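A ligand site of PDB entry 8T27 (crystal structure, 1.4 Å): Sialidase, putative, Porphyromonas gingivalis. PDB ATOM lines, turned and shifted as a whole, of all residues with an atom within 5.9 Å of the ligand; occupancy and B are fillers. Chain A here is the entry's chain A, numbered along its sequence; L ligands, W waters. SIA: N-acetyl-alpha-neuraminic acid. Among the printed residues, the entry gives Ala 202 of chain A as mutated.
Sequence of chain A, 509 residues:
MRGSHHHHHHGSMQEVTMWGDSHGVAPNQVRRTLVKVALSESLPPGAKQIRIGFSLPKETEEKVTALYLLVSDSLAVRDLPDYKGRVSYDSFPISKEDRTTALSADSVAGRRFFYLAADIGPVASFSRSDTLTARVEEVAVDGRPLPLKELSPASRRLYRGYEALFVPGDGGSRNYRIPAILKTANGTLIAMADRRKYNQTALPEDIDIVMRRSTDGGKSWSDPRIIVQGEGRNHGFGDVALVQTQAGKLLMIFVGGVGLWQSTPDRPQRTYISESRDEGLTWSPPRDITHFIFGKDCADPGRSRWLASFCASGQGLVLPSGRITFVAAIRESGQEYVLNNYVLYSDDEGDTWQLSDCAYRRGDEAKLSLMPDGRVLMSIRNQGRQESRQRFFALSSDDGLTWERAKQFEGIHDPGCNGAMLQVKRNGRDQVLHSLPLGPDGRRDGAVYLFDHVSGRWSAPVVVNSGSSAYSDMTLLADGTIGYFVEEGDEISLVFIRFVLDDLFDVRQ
Ile 178 touches the ligand.
CG2 of Val 255 touches C11 of the ligand, 3.95 Å away.
Leu 260 touches the ligand.
NE2 of Gln 269 touches C11 of the ligand, 3.98 Å away.
CZ of Phe 310 touches O8 of the ligand, 3.5 Å away.
Gln 383 touches the ligand.
14 residues have an atom within 4 Å of the ligand: Arg 177, Ile 178, Arg 196, Asp 239, Val 255, Leu 260, Gln 269, Phe 310, Asp 364, Glu 365, Arg 381, Gln 383, Arg 443 and Tyr 471.
The backbone NH (N) of Tyr 471 lies within hydrogen-bond range of the side-chain carboxylate (OE1) of Glu 487 (2.8 Å).
O of Arg 177 is in hydrogen-bond range of N of Asp 194 (2.8 Å).
The backbone carbonyl oxygen (O) of Gly 416 lies within hydrogen-bond range of the guanidinium group (NH2) of Arg 443 (2.9 Å).
The guanidinium group (NE) of Arg 381 is in salt-bridge range of the side-chain carboxylate (OD1) of Asp 364 (3.6 Å).
The guanidinium group (NH2) of Arg 381 lies within hydrogen-bond range of the side-chain amide oxygen (OE1) of Gln 383, 2.8 Å away.
The side-chain hydroxyl (OH) of Tyr 471 lies within hydrogen-bond range of the guanidinium group (NH1) of Arg 381, at 3.0 Å.
OE2 of Glu 487 sits at hydrogen-bond distance from N of Ile 178 (2.8 Å).
The side-chain hydroxyl (OH) of Tyr 471 lies within hydrogen-bond range of the side-chain carboxylate (OE2) of Glu 365, 2.6 Å away.
Water W3 lies within hydrogen-bond range of O10 of the ligand (2.6 Å), N of Leu 260 (2.9 Å) and O of Leu 203 (3.0 Å).
Water W5 lies within hydrogen-bond range of an oxygen (O2) of the ligand (2.6 Å), the guanidinium group of Arg 196 (2.9 Å) and the guanidinium group of Arg 177 (3.1 Å).
Water W1 lies within hydrogen-bond range of an oxygen (O7) of the ligand (2.8 Å) and the indole nitrogen of Trp 261 (3.3 Å).
Water W4 bridges N of Leu 203 (3.0 Å) and O4 of the ligand (3.2 Å).
The guanidinium group of Arg 443 lies within salt-bridge range of an oxygen (O1B) of the ligand (2.9 Å).
O4 of the ligand is in hydrogen-bond range of NH2 of Arg 196, at 2.9 Å.
An oxygen (O8) of the ligand is in hydrogen-bond range of the side-chain carboxylate of Glu 365 (3.5 Å).
An oxygen (O1B) of the ligand is in salt-bridge range of the guanidinium group (NH2) of Arg 381, 3.0 Å away.
The guanidinium group (NH1) of Arg 177 lies within salt-bridge range of an oxygen (O1A) of the ligand (2.8 Å).
The side-chain carboxylate (OD2) of Asp 364 lies within hydrogen-bond range of an oxygen (O9) of the ligand.
OD2 of Asp 239 sits at hydrogen-bond distance from N5 of the ligand.
OH of Tyr 471 sits close to O6 of the ligand (3.1 Å).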
ATOM      1  N   ARG A 177      15.086 -36.196   8.451  1.00  0.00           N
ATOM      2  CA  ARG A 177      14.448 -34.878   8.317  1.00  0.00           C
ATOM      3  C   ARG A 177      13.955 -34.750   6.882  1.00  0.00           C
ATOM      4  O   ARG A 177      14.288 -35.562   6.009  1.00  0.00           O
ATOM      5  CB  ARG A 177      15.453 -33.720   8.594  1.00  0.00           C
ATOM      6  CG  ARG A 177      15.580 -33.374  10.138  1.00  0.00           C
ATOM      7  CD  ARG A 177      15.967 -31.911  10.366  1.00  0.00           C
ATOM      8  NE  ARG A 177      14.864 -31.084   9.909  1.00  0.00           N
ATOM      9  CZ  ARG A 177      14.957 -29.792   9.573  1.00  0.00           C
ATOM     10  NH1 ARG A 177      16.102 -29.114   9.670  1.00  0.00           N
ATOM     11  NH2 ARG A 177      13.852 -29.151   9.119  1.00  0.00           N
ATOM     12  N   ILE A 178      13.122 -33.736   6.663  1.00  0.00           N
ATOM     13  CA  ILE A 178      12.857 -33.154   5.330  1.00  0.00           C
ATOM     14  C   ILE A 178      11.844 -34.025   4.559  1.00  0.00           C
ATOM     15  O   ILE A 178      12.201 -34.743   3.652  1.00  0.00           O
ATOM     16  CB  ILE A 178      14.133 -32.862   4.500  1.00  0.00           C
ATOM     17  CG1 ILE A 178      15.263 -32.239   5.291  1.00  0.00           C
ATOM     18  CG2 ILE A 178      13.674 -31.936   3.334  1.00  0.00           C
ATOM     19  CD1 ILE A 178      14.814 -30.890   6.009  1.00  0.00           C
ATOM     20  N   ASP A 194      15.265 -37.053   3.862  1.00  0.00           N
ATOM     21  CA  ASP A 194      16.694 -37.110   4.121  1.00  0.00           C
ATOM     22  C   ASP A 194      16.969 -38.166   5.203  1.00  0.00           C
ATOM     23  O   ASP A 194      16.438 -38.101   6.328  1.00  0.00           O
ATOM     24  CB  ASP A 194      17.229 -35.810   4.697  1.00  0.00           C
ATOM     25  CG  ASP A 194      17.389 -34.642   3.778  1.00  0.00           C
ATOM     26  OD1 ASP A 194      16.843 -34.558   2.661  1.00  0.00           O
ATOM     27  OD2 ASP A 194      18.257 -33.789   4.173  1.00  0.00           O
ATOM     28  N   ARG A 196      19.489 -38.765   7.488  1.00  0.00           N
ATOM     29  CA  ARG A 196      20.526 -37.951   8.119  1.00  0.00           C
ATOM     30  C   ARG A 196      21.311 -38.898   9.046  1.00  0.00           C
ATOM     31  O   ARG A 196      21.121 -38.960  10.273  1.00  0.00           O
ATOM     32  CB  ARG A 196      19.876 -36.759   8.827  1.00  0.00           C
ATOM     33  CG  ARG A 196      19.268 -35.779   7.743  1.00  0.00           C
ATOM     34  CD  ARG A 196      19.282 -34.350   8.131  1.00  0.00           C
ATOM     35  NE  ARG A 196      18.896 -33.494   7.008  1.00  0.00           N
ATOM     36  CZ  ARG A 196      18.823 -32.168   7.074  1.00  0.00           C
ATOM     37  NH1 ARG A 196      19.045 -31.474   8.189  1.00  0.00           N
ATOM     38  NH2 ARG A 196      18.516 -31.491   5.964  1.00  0.00           N
ATOM     39  N   ALA A 202      22.415 -30.267   8.179  1.00  0.00           N
ATOM     40  CA  ALA A 202      22.153 -30.153   6.757  1.00  0.00           C
ATOM     41  C   ALA A 202      23.402 -30.464   5.931  1.00  0.00           C
ATOM     42  O   ALA A 202      24.518 -30.620   6.473  1.00  0.00           O
ATOM     43  CB  ALA A 202      21.792 -28.698   6.473  1.00  0.00           C
ATOM     44  N   LEU A 203      23.222 -30.498   4.599  1.00  0.00           N
ATOM     45  CA  LEU A 203      24.395 -30.418   3.731  1.00  0.00           C
ATOM     46  C   LEU A 203      25.270 -29.238   4.181  1.00  0.00           C
ATOM     47  O   LEU A 203      24.732 -28.164   4.474  1.00  0.00           O
ATOM     48  CB  LEU A 203      23.954 -30.192   2.264  1.00  0.00           C
ATOM     49  CG  LEU A 203      23.097 -31.334   1.687  1.00  0.00           C
ATOM     50  CD1 LEU A 203      22.471 -30.876   0.409  1.00  0.00           C
ATOM     51  CD2 LEU A 203      23.864 -32.697   1.498  1.00  0.00           C
ATOM     52  N   ASP A 239      16.957 -32.778   0.423  1.00  0.00           N
ATOM     53  CA  ASP A 239      15.910 -31.798   0.099  1.00  0.00           C
ATOM     54  C   ASP A 239      15.157 -32.211  -1.171  1.00  0.00           C
ATOM     55  O   ASP A 239      15.175 -31.536  -2.194  1.00  0.00           O
ATOM     56  CB  ASP A 239      16.489 -30.371  -0.050  1.00  0.00           C
ATOM     57  CG  ASP A 239      16.633 -29.629   1.333  1.00  0.00           C
ATOM     58  OD1 ASP A 239      17.097 -30.282   2.275  1.00  0.00           O
ATOM     59  OD2 ASP A 239      16.264 -28.449   1.466  1.00  0.00           O
ATOM     60  N   VAL A 255      19.051 -31.636  -4.184  1.00  0.00           N
ATOM     61  CA  VAL A 255      20.362 -31.060  -4.261  1.00  0.00           C
ATOM     62  C   VAL A 255      21.396 -32.025  -3.726  1.00  0.00           C
ATOM     63  O   VAL A 255      21.109 -32.990  -2.995  1.00  0.00           O
ATOM     64  CB  VAL A 255      20.471 -29.713  -3.548  1.00  0.00           C
ATOM     65  CG1 VAL A 255      19.777 -28.638  -4.332  1.00  0.00           C
ATOM     66  CG2 VAL A 255      19.947 -29.703  -2.104  1.00  0.00           C
ATOM     67  N   GLY A 259      27.257 -27.131   1.271  1.00  0.00           N
ATOM     68  CA  GLY A 259      26.128 -26.400   1.832  1.00  0.00           C
ATOM     69  C   GLY A 259      25.658 -25.250   0.963  1.00  0.00           C
ATOM     70  O   GLY A 259      26.388 -24.747   0.110  1.00  0.00           O
ATOM     71  N   LEU A 260      24.399 -24.848   1.156  1.00  0.00           N
ATOM     72  CA  LEU A 260      23.808 -23.787   0.358  1.00  0.00           C
ATOM     73  C   LEU A 260      24.693 -22.536   0.344  1.00  0.00           C
ATOM     74  O   LEU A 260      24.903 -21.916  -0.714  1.00  0.00           O
ATOM     75  CB  LEU A 260      22.440 -23.449   0.999  1.00  0.00           C
ATOM     76  CG  LEU A 260      21.655 -22.294   0.351  1.00  0.00           C
ATOM     77  CD1 LEU A 260      21.302 -22.650  -1.028  1.00  0.00           C
ATOM     78  CD2 LEU A 260      20.394 -22.132   1.327  1.00  0.00           C
ATOM     79  N   TRP A 261      25.204 -22.142   1.502  1.00  0.00           N
ATOM     80  CA  TRP A 261      25.963 -20.883   1.573  1.00  0.00           C
ATOM     81  C   TRP A 261      27.409 -21.064   1.180  1.00  0.00           C
ATOM     82  O   TRP A 261      28.143 -20.054   1.077  1.00  0.00           O
ATOM     83  CB  TRP A 261      25.867 -20.244   2.982  1.00  0.00           C
ATOM     84  CG  TRP A 261      24.416 -20.054   3.352  1.00  0.00           C
ATOM     85  CD1 TRP A 261      23.727 -20.722   4.332  1.00  0.00           C
ATOM     86  CD2 TRP A 261      23.477 -19.138   2.757  1.00  0.00           C
ATOM     87  NE1 TRP A 261      22.428 -20.296   4.362  1.00  0.00           N
ATOM     88  CE2 TRP A 261      22.238 -19.330   3.410  1.00  0.00           C
ATOM     89  CE3 TRP A 261      23.545 -18.222   1.686  1.00  0.00           C
ATOM     90  CZ2 TRP A 261      21.104 -18.587   3.108  1.00  0.00           C
ATOM     91  CZ3 TRP A 261      22.385 -17.477   1.359  1.00  0.00           C
ATOM     92  CH2 TRP A 261      21.187 -17.668   2.079  1.00  0.00           C
ATOM     93  N   GLN A 269      26.782 -26.345  -5.186  1.00  0.00           N
ATOM     94  CA  GLN A 269      25.840 -27.347  -4.703  1.00  0.00           C
ATOM     95  C   GLN A 269      24.856 -27.599  -5.840  1.00  0.00           C
ATOM     96  O   GLN A 269      24.186 -26.667  -6.308  1.00  0.00           O
ATOM     97  CB  GLN A 269      25.104 -26.820  -3.465  1.00  0.00           C
ATOM     98  CG  GLN A 269      23.926 -27.699  -3.036  1.00  0.00           C
ATOM     99  CD  GLN A 269      23.050 -27.011  -2.011  1.00  0.00           C
ATOM    100  OE1 GLN A 269      22.203 -26.211  -2.367  1.00  0.00           O
ATOM    101  NE2 GLN A 269      23.248 -27.317  -0.718  1.00  0.00           N
ATOM    102  N   PHE A 310      18.273 -23.890  -4.668  1.00  0.00           N
ATOM    103  CA  PHE A 310      17.649 -25.158  -4.277  1.00  0.00           C
ATOM    104  C   PHE A 310      16.133 -25.051  -4.393  1.00  0.00           C
ATOM    105  O   PHE A 310      15.525 -24.013  -4.092  1.00  0.00           O
ATOM    106  CB  PHE A 310      18.059 -25.676  -2.874  1.00  0.00           C
ATOM    107  CG  PHE A 310      17.434 -24.945  -1.709  1.00  0.00           C
ATOM    108  CD1 PHE A 310      17.749 -23.590  -1.471  1.00  0.00           C
ATOM    109  CD2 PHE A 310      16.588 -25.633  -0.798  1.00  0.00           C
ATOM    110  CE1 PHE A 310      17.191 -22.971  -0.338  1.00  0.00           C
ATOM    111  CE2 PHE A 310      16.037 -24.985   0.331  1.00  0.00           C
ATOM    112  CZ  PHE A 310      16.384 -23.638   0.554  1.00  0.00           C
ATOM    113  N   LEU A 339      18.228 -14.820  -0.594  1.00  0.00           N
ATOM    114  CA  LEU A 339      17.811 -15.602  -1.740  1.00  0.00           C
ATOM    115  C   LEU A 339      16.668 -14.925  -2.483  1.00  0.00           C
ATOM    116  O   LEU A 339      15.875 -14.224  -1.870  1.00  0.00           O
ATOM    117  CB  LEU A 339      17.313 -16.979  -1.291  1.00  0.00           C
ATOM    118  CG  LEU A 339      18.350 -17.743  -0.444  1.00  0.00           C
ATOM    119  CD1 LEU A 339      17.710 -19.026   0.091  1.00  0.00           C
ATOM    120  CD2 LEU A 339      19.522 -18.115  -1.301  1.00  0.00           C
ATOM    121  N   ASP A 364      12.653 -17.439   0.179  1.00  0.00           N
ATOM    122  CA  ASP A 364      13.225 -18.644   0.755  1.00  0.00           C
ATOM    123  C   ASP A 364      12.347 -19.795   0.228  1.00  0.00           C
ATOM    124  O   ASP A 364      11.710 -19.628  -0.814  1.00  0.00           O
ATOM    125  CB  ASP A 364      13.258 -18.601   2.290  1.00  0.00           C
ATOM    126  CG  ASP A 364      14.374 -19.486   2.853  1.00  0.00           C
ATOM    127  OD1 ASP A 364      14.194 -20.732   2.901  1.00  0.00           O
ATOM    128  OD2 ASP A 364      15.489 -18.983   3.244  1.00  0.00           O
ATOM    129  N   GLU A 365      12.325 -20.972   0.870  1.00  0.00           N
ATOM    130  CA  GLU A 365      11.546 -22.102   0.333  1.00  0.00           C
ATOM    131  C   GLU A 365      10.134 -21.667   0.006  1.00  0.00           C
ATOM    132  O   GLU A 365       9.427 -21.123   0.856  1.00  0.00           O
ATOM    133  CB  GLU A 365      11.446 -23.186   1.409  1.00  0.00           C
ATOM    134  CG  GLU A 365      12.795 -23.894   1.694  1.00  0.00           C
ATOM    135  CD  GLU A 365      12.804 -24.589   3.022  1.00  0.00           C
ATOM    136  OE1 GLU A 365      11.986 -24.171   3.910  1.00  0.00           O
ATOM    137  OE2 GLU A 365      13.640 -25.507   3.203  1.00  0.00           O
ATOM    138  N   ARG A 381       8.262 -18.875   2.367  1.00  0.00           N
ATOM    139  CA  ARG A 381       8.817 -18.803   3.713  1.00  0.00           C
ATOM    140  C   ARG A 381       9.418 -17.428   3.986  1.00  0.00           C
ATOM    141  O   ARG A 381      10.214 -16.885   3.208  1.00  0.00           O
ATOM    142  CB  ARG A 381       9.871 -19.915   3.857  1.00  0.00           C
ATOM    143  CG  ARG A 381      10.723 -19.838   5.161  1.00  0.00           C
ATOM    144  CD  ARG A 381      11.585 -21.119   5.227  1.00  0.00           C
ATOM    145  NE  ARG A 381      12.689 -20.953   6.170  1.00  0.00           N
ATOM    146  CZ  ARG A 381      13.400 -21.982   6.600  1.00  0.00           C
ATOM    147  NH1 ARG A 381      13.120 -23.221   6.223  1.00  0.00           N
ATOM    148  NH2 ARG A 381      14.428 -21.764   7.441  1.00  0.00           N
ATOM    149  N   GLN A 383      12.106 -15.762   5.850  1.00  0.00           N
ATOM    150  CA  GLN A 383      13.402 -16.084   6.488  1.00  0.00           C
ATOM    151  C   GLN A 383      14.011 -14.803   7.037  1.00  0.00           C
ATOM    152  O   GLN A 383      14.033 -13.789   6.342  1.00  0.00           O
ATOM    153  CB  GLN A 383      14.335 -16.781   5.483  1.00  0.00           C
ATOM    154  CG  GLN A 383      15.701 -17.192   6.044  1.00  0.00           C
ATOM    155  CD  GLN A 383      15.595 -18.241   7.134  1.00  0.00           C
ATOM    156  OE1 GLN A 383      14.617 -18.992   7.187  1.00  0.00           O
ATOM    157  NE2 GLN A 383      16.569 -18.271   8.034  1.00  0.00           N
ATOM    158  N   GLY A 416       9.409 -19.132  10.205  1.00  0.00           N
ATOM    159  CA  GLY A 416      10.488 -19.303   9.257  1.00  0.00           C
ATOM    160  C   GLY A 416      10.660 -20.783   8.997  1.00  0.00           C
ATOM    161  O   GLY A 416      11.659 -21.380   9.398  1.00  0.00           O
ATOM    162  N   ARG A 443       9.580 -23.448  16.258  1.00  0.00           N
ATOM    163  CA  ARG A 443       9.016 -24.590  15.537  1.00  0.00           C
ATOM    164  C   ARG A 443       8.285 -25.486  16.522  1.00  0.00           C
ATOM    165  O   ARG A 443       8.813 -26.498  17.016  1.00  0.00           O
ATOM    166  CB  ARG A 443      10.142 -25.288  14.784  1.00  0.00           C
ATOM    167  CG  ARG A 443      10.458 -24.530  13.489  1.00  0.00           C
ATOM    168  CD  ARG A 443      11.706 -24.994  12.875  1.00  0.00           C
ATOM    169  NE  ARG A 443      12.052 -24.170  11.716  1.00  0.00           N
ATOM    170  CZ  ARG A 443      12.884 -24.606  10.792  1.00  0.00           C
ATOM    171  NH1 ARG A 443      13.389 -25.828  10.839  1.00  0.00           N
ATOM    172  NH2 ARG A 443      13.197 -23.813   9.788  1.00  0.00           N
ATOM    173  N   TYR A 471       9.017 -29.015   9.461  1.00  0.00           N
ATOM    174  CA  TYR A 471       8.527 -29.045   8.075  1.00  0.00           C
ATOM    175  C   TYR A 471       7.336 -29.969   7.935  1.00  0.00           C
ATOM    176  O   TYR A 471       7.207 -30.977   8.655  1.00  0.00           O
ATOM    177  CB  TYR A 471       9.632 -29.632   7.145  1.00  0.00           C
ATOM    178  CG  TYR A 471      10.760 -28.668   6.797  1.00  0.00           C
ATOM    179  CD1 TYR A 471      11.071 -27.583   7.617  1.00  0.00           C
ATOM    180  CD2 TYR A 471      11.528 -28.866   5.657  1.00  0.00           C
ATOM    181  CE1 TYR A 471      12.083 -26.699   7.267  1.00  0.00           C
ATOM    182  CE2 TYR A 471      12.515 -28.034   5.273  1.00  0.00           C
ATOM    183  CZ  TYR A 471      12.826 -26.899   6.083  1.00  0.00           C
ATOM    184  OH  TYR A 471      13.823 -26.043   5.727  1.00  0.00           O
ATOM    185  N   GLU A 487       7.398 -33.246  10.531  1.00  0.00           N
ATOM    186  CA  GLU A 487       8.538 -33.446  11.423  1.00  0.00           C
ATOM    187  C   GLU A 487       8.089 -33.256  12.865  1.00  0.00           C
ATOM    188  O   GLU A 487       7.939 -32.115  13.303  1.00  0.00           O
ATOM    189  CB  GLU A 487       9.631 -32.431  11.092  1.00  0.00           C
ATOM    190  CG  GLU A 487      10.159 -32.599   9.698  1.00  0.00           C
ATOM    191  CD  GLU A 487      11.409 -31.816   9.472  1.00  0.00           C
ATOM    192  OE1 GLU A 487      11.395 -30.567   9.652  1.00  0.00           O
ATOM    193  OE2 GLU A 487      12.486 -32.360   9.053  1.00  0.00           O
HETATM  194  C1  SIA L   1      15.750 -25.744   7.960  1.00  0.00           C
HETATM  195  C2  SIA L   1      16.731 -26.169   6.840  1.00  0.00           C
HETATM  196  C3  SIA L   1      16.470 -27.518   6.177  1.00  0.00           C
HETATM  197  C4  SIA L   1      16.891 -27.742   4.748  1.00  0.00           C
HETATM  198  C5  SIA L   1      17.778 -26.635   4.269  1.00  0.00           C
HETATM  199  C6  SIA L   1      17.031 -25.313   4.417  1.00  0.00           C
HETATM  200  C7  SIA L   1      17.821 -24.065   3.991  1.00  0.00           C
HETATM  201  C8  SIA L   1      17.103 -22.753   4.380  1.00  0.00           C
HETATM  202  C9  SIA L   1      17.803 -21.517   3.749  1.00  0.00           C
HETATM  203  C10 SIA L   1      19.415 -26.624   2.298  1.00  0.00           C
HETATM  204  C11 SIA L   1      19.598 -27.101   0.851  1.00  0.00           C
HETATM  205  N5  SIA L   1      18.119 -26.944   2.854  1.00  0.00           N
HETATM  206  O1A SIA L   1      15.304 -26.551   8.763  1.00  0.00           O
HETATM  207  O1B SIA L   1      15.440 -24.536   8.148  1.00  0.00           O
HETATM  208  O2  SIA L   1      18.004 -26.204   7.371  1.00  0.00           O
HETATM  209  O4  SIA L   1      17.667 -29.009   4.727  1.00  0.00           O
HETATM  210  O6  SIA L   1      16.759 -25.057   5.851  1.00  0.00           O
HETATM  211  O7  SIA L   1      19.121 -24.001   4.528  1.00  0.00           O
HETATM  212  O8  SIA L   1      15.767 -22.840   3.914  1.00  0.00           O
HETATM  213  O9  SIA L   1      17.364 -20.306   4.391  1.00  0.00           O
HETATM  214  O10 SIA L   1      20.272 -26.049   2.948  1.00  0.00           O
HETATM  215  O   HOH W   1      20.363 -22.115   6.223  1.00  0.00           O
HETATM  216  O   HOH W   2      17.623 -22.823   8.435  1.00  0.00           O
HETATM  217  O   HOH W   3      22.838 -26.625   2.762  1.00  0.00           O
HETATM  218  O   HOH W   4      20.545 -29.720   3.542  1.00  0.00           O
HETATM  219  O   HOH W   5      18.848 -28.556   8.235  1.00  0.00           O
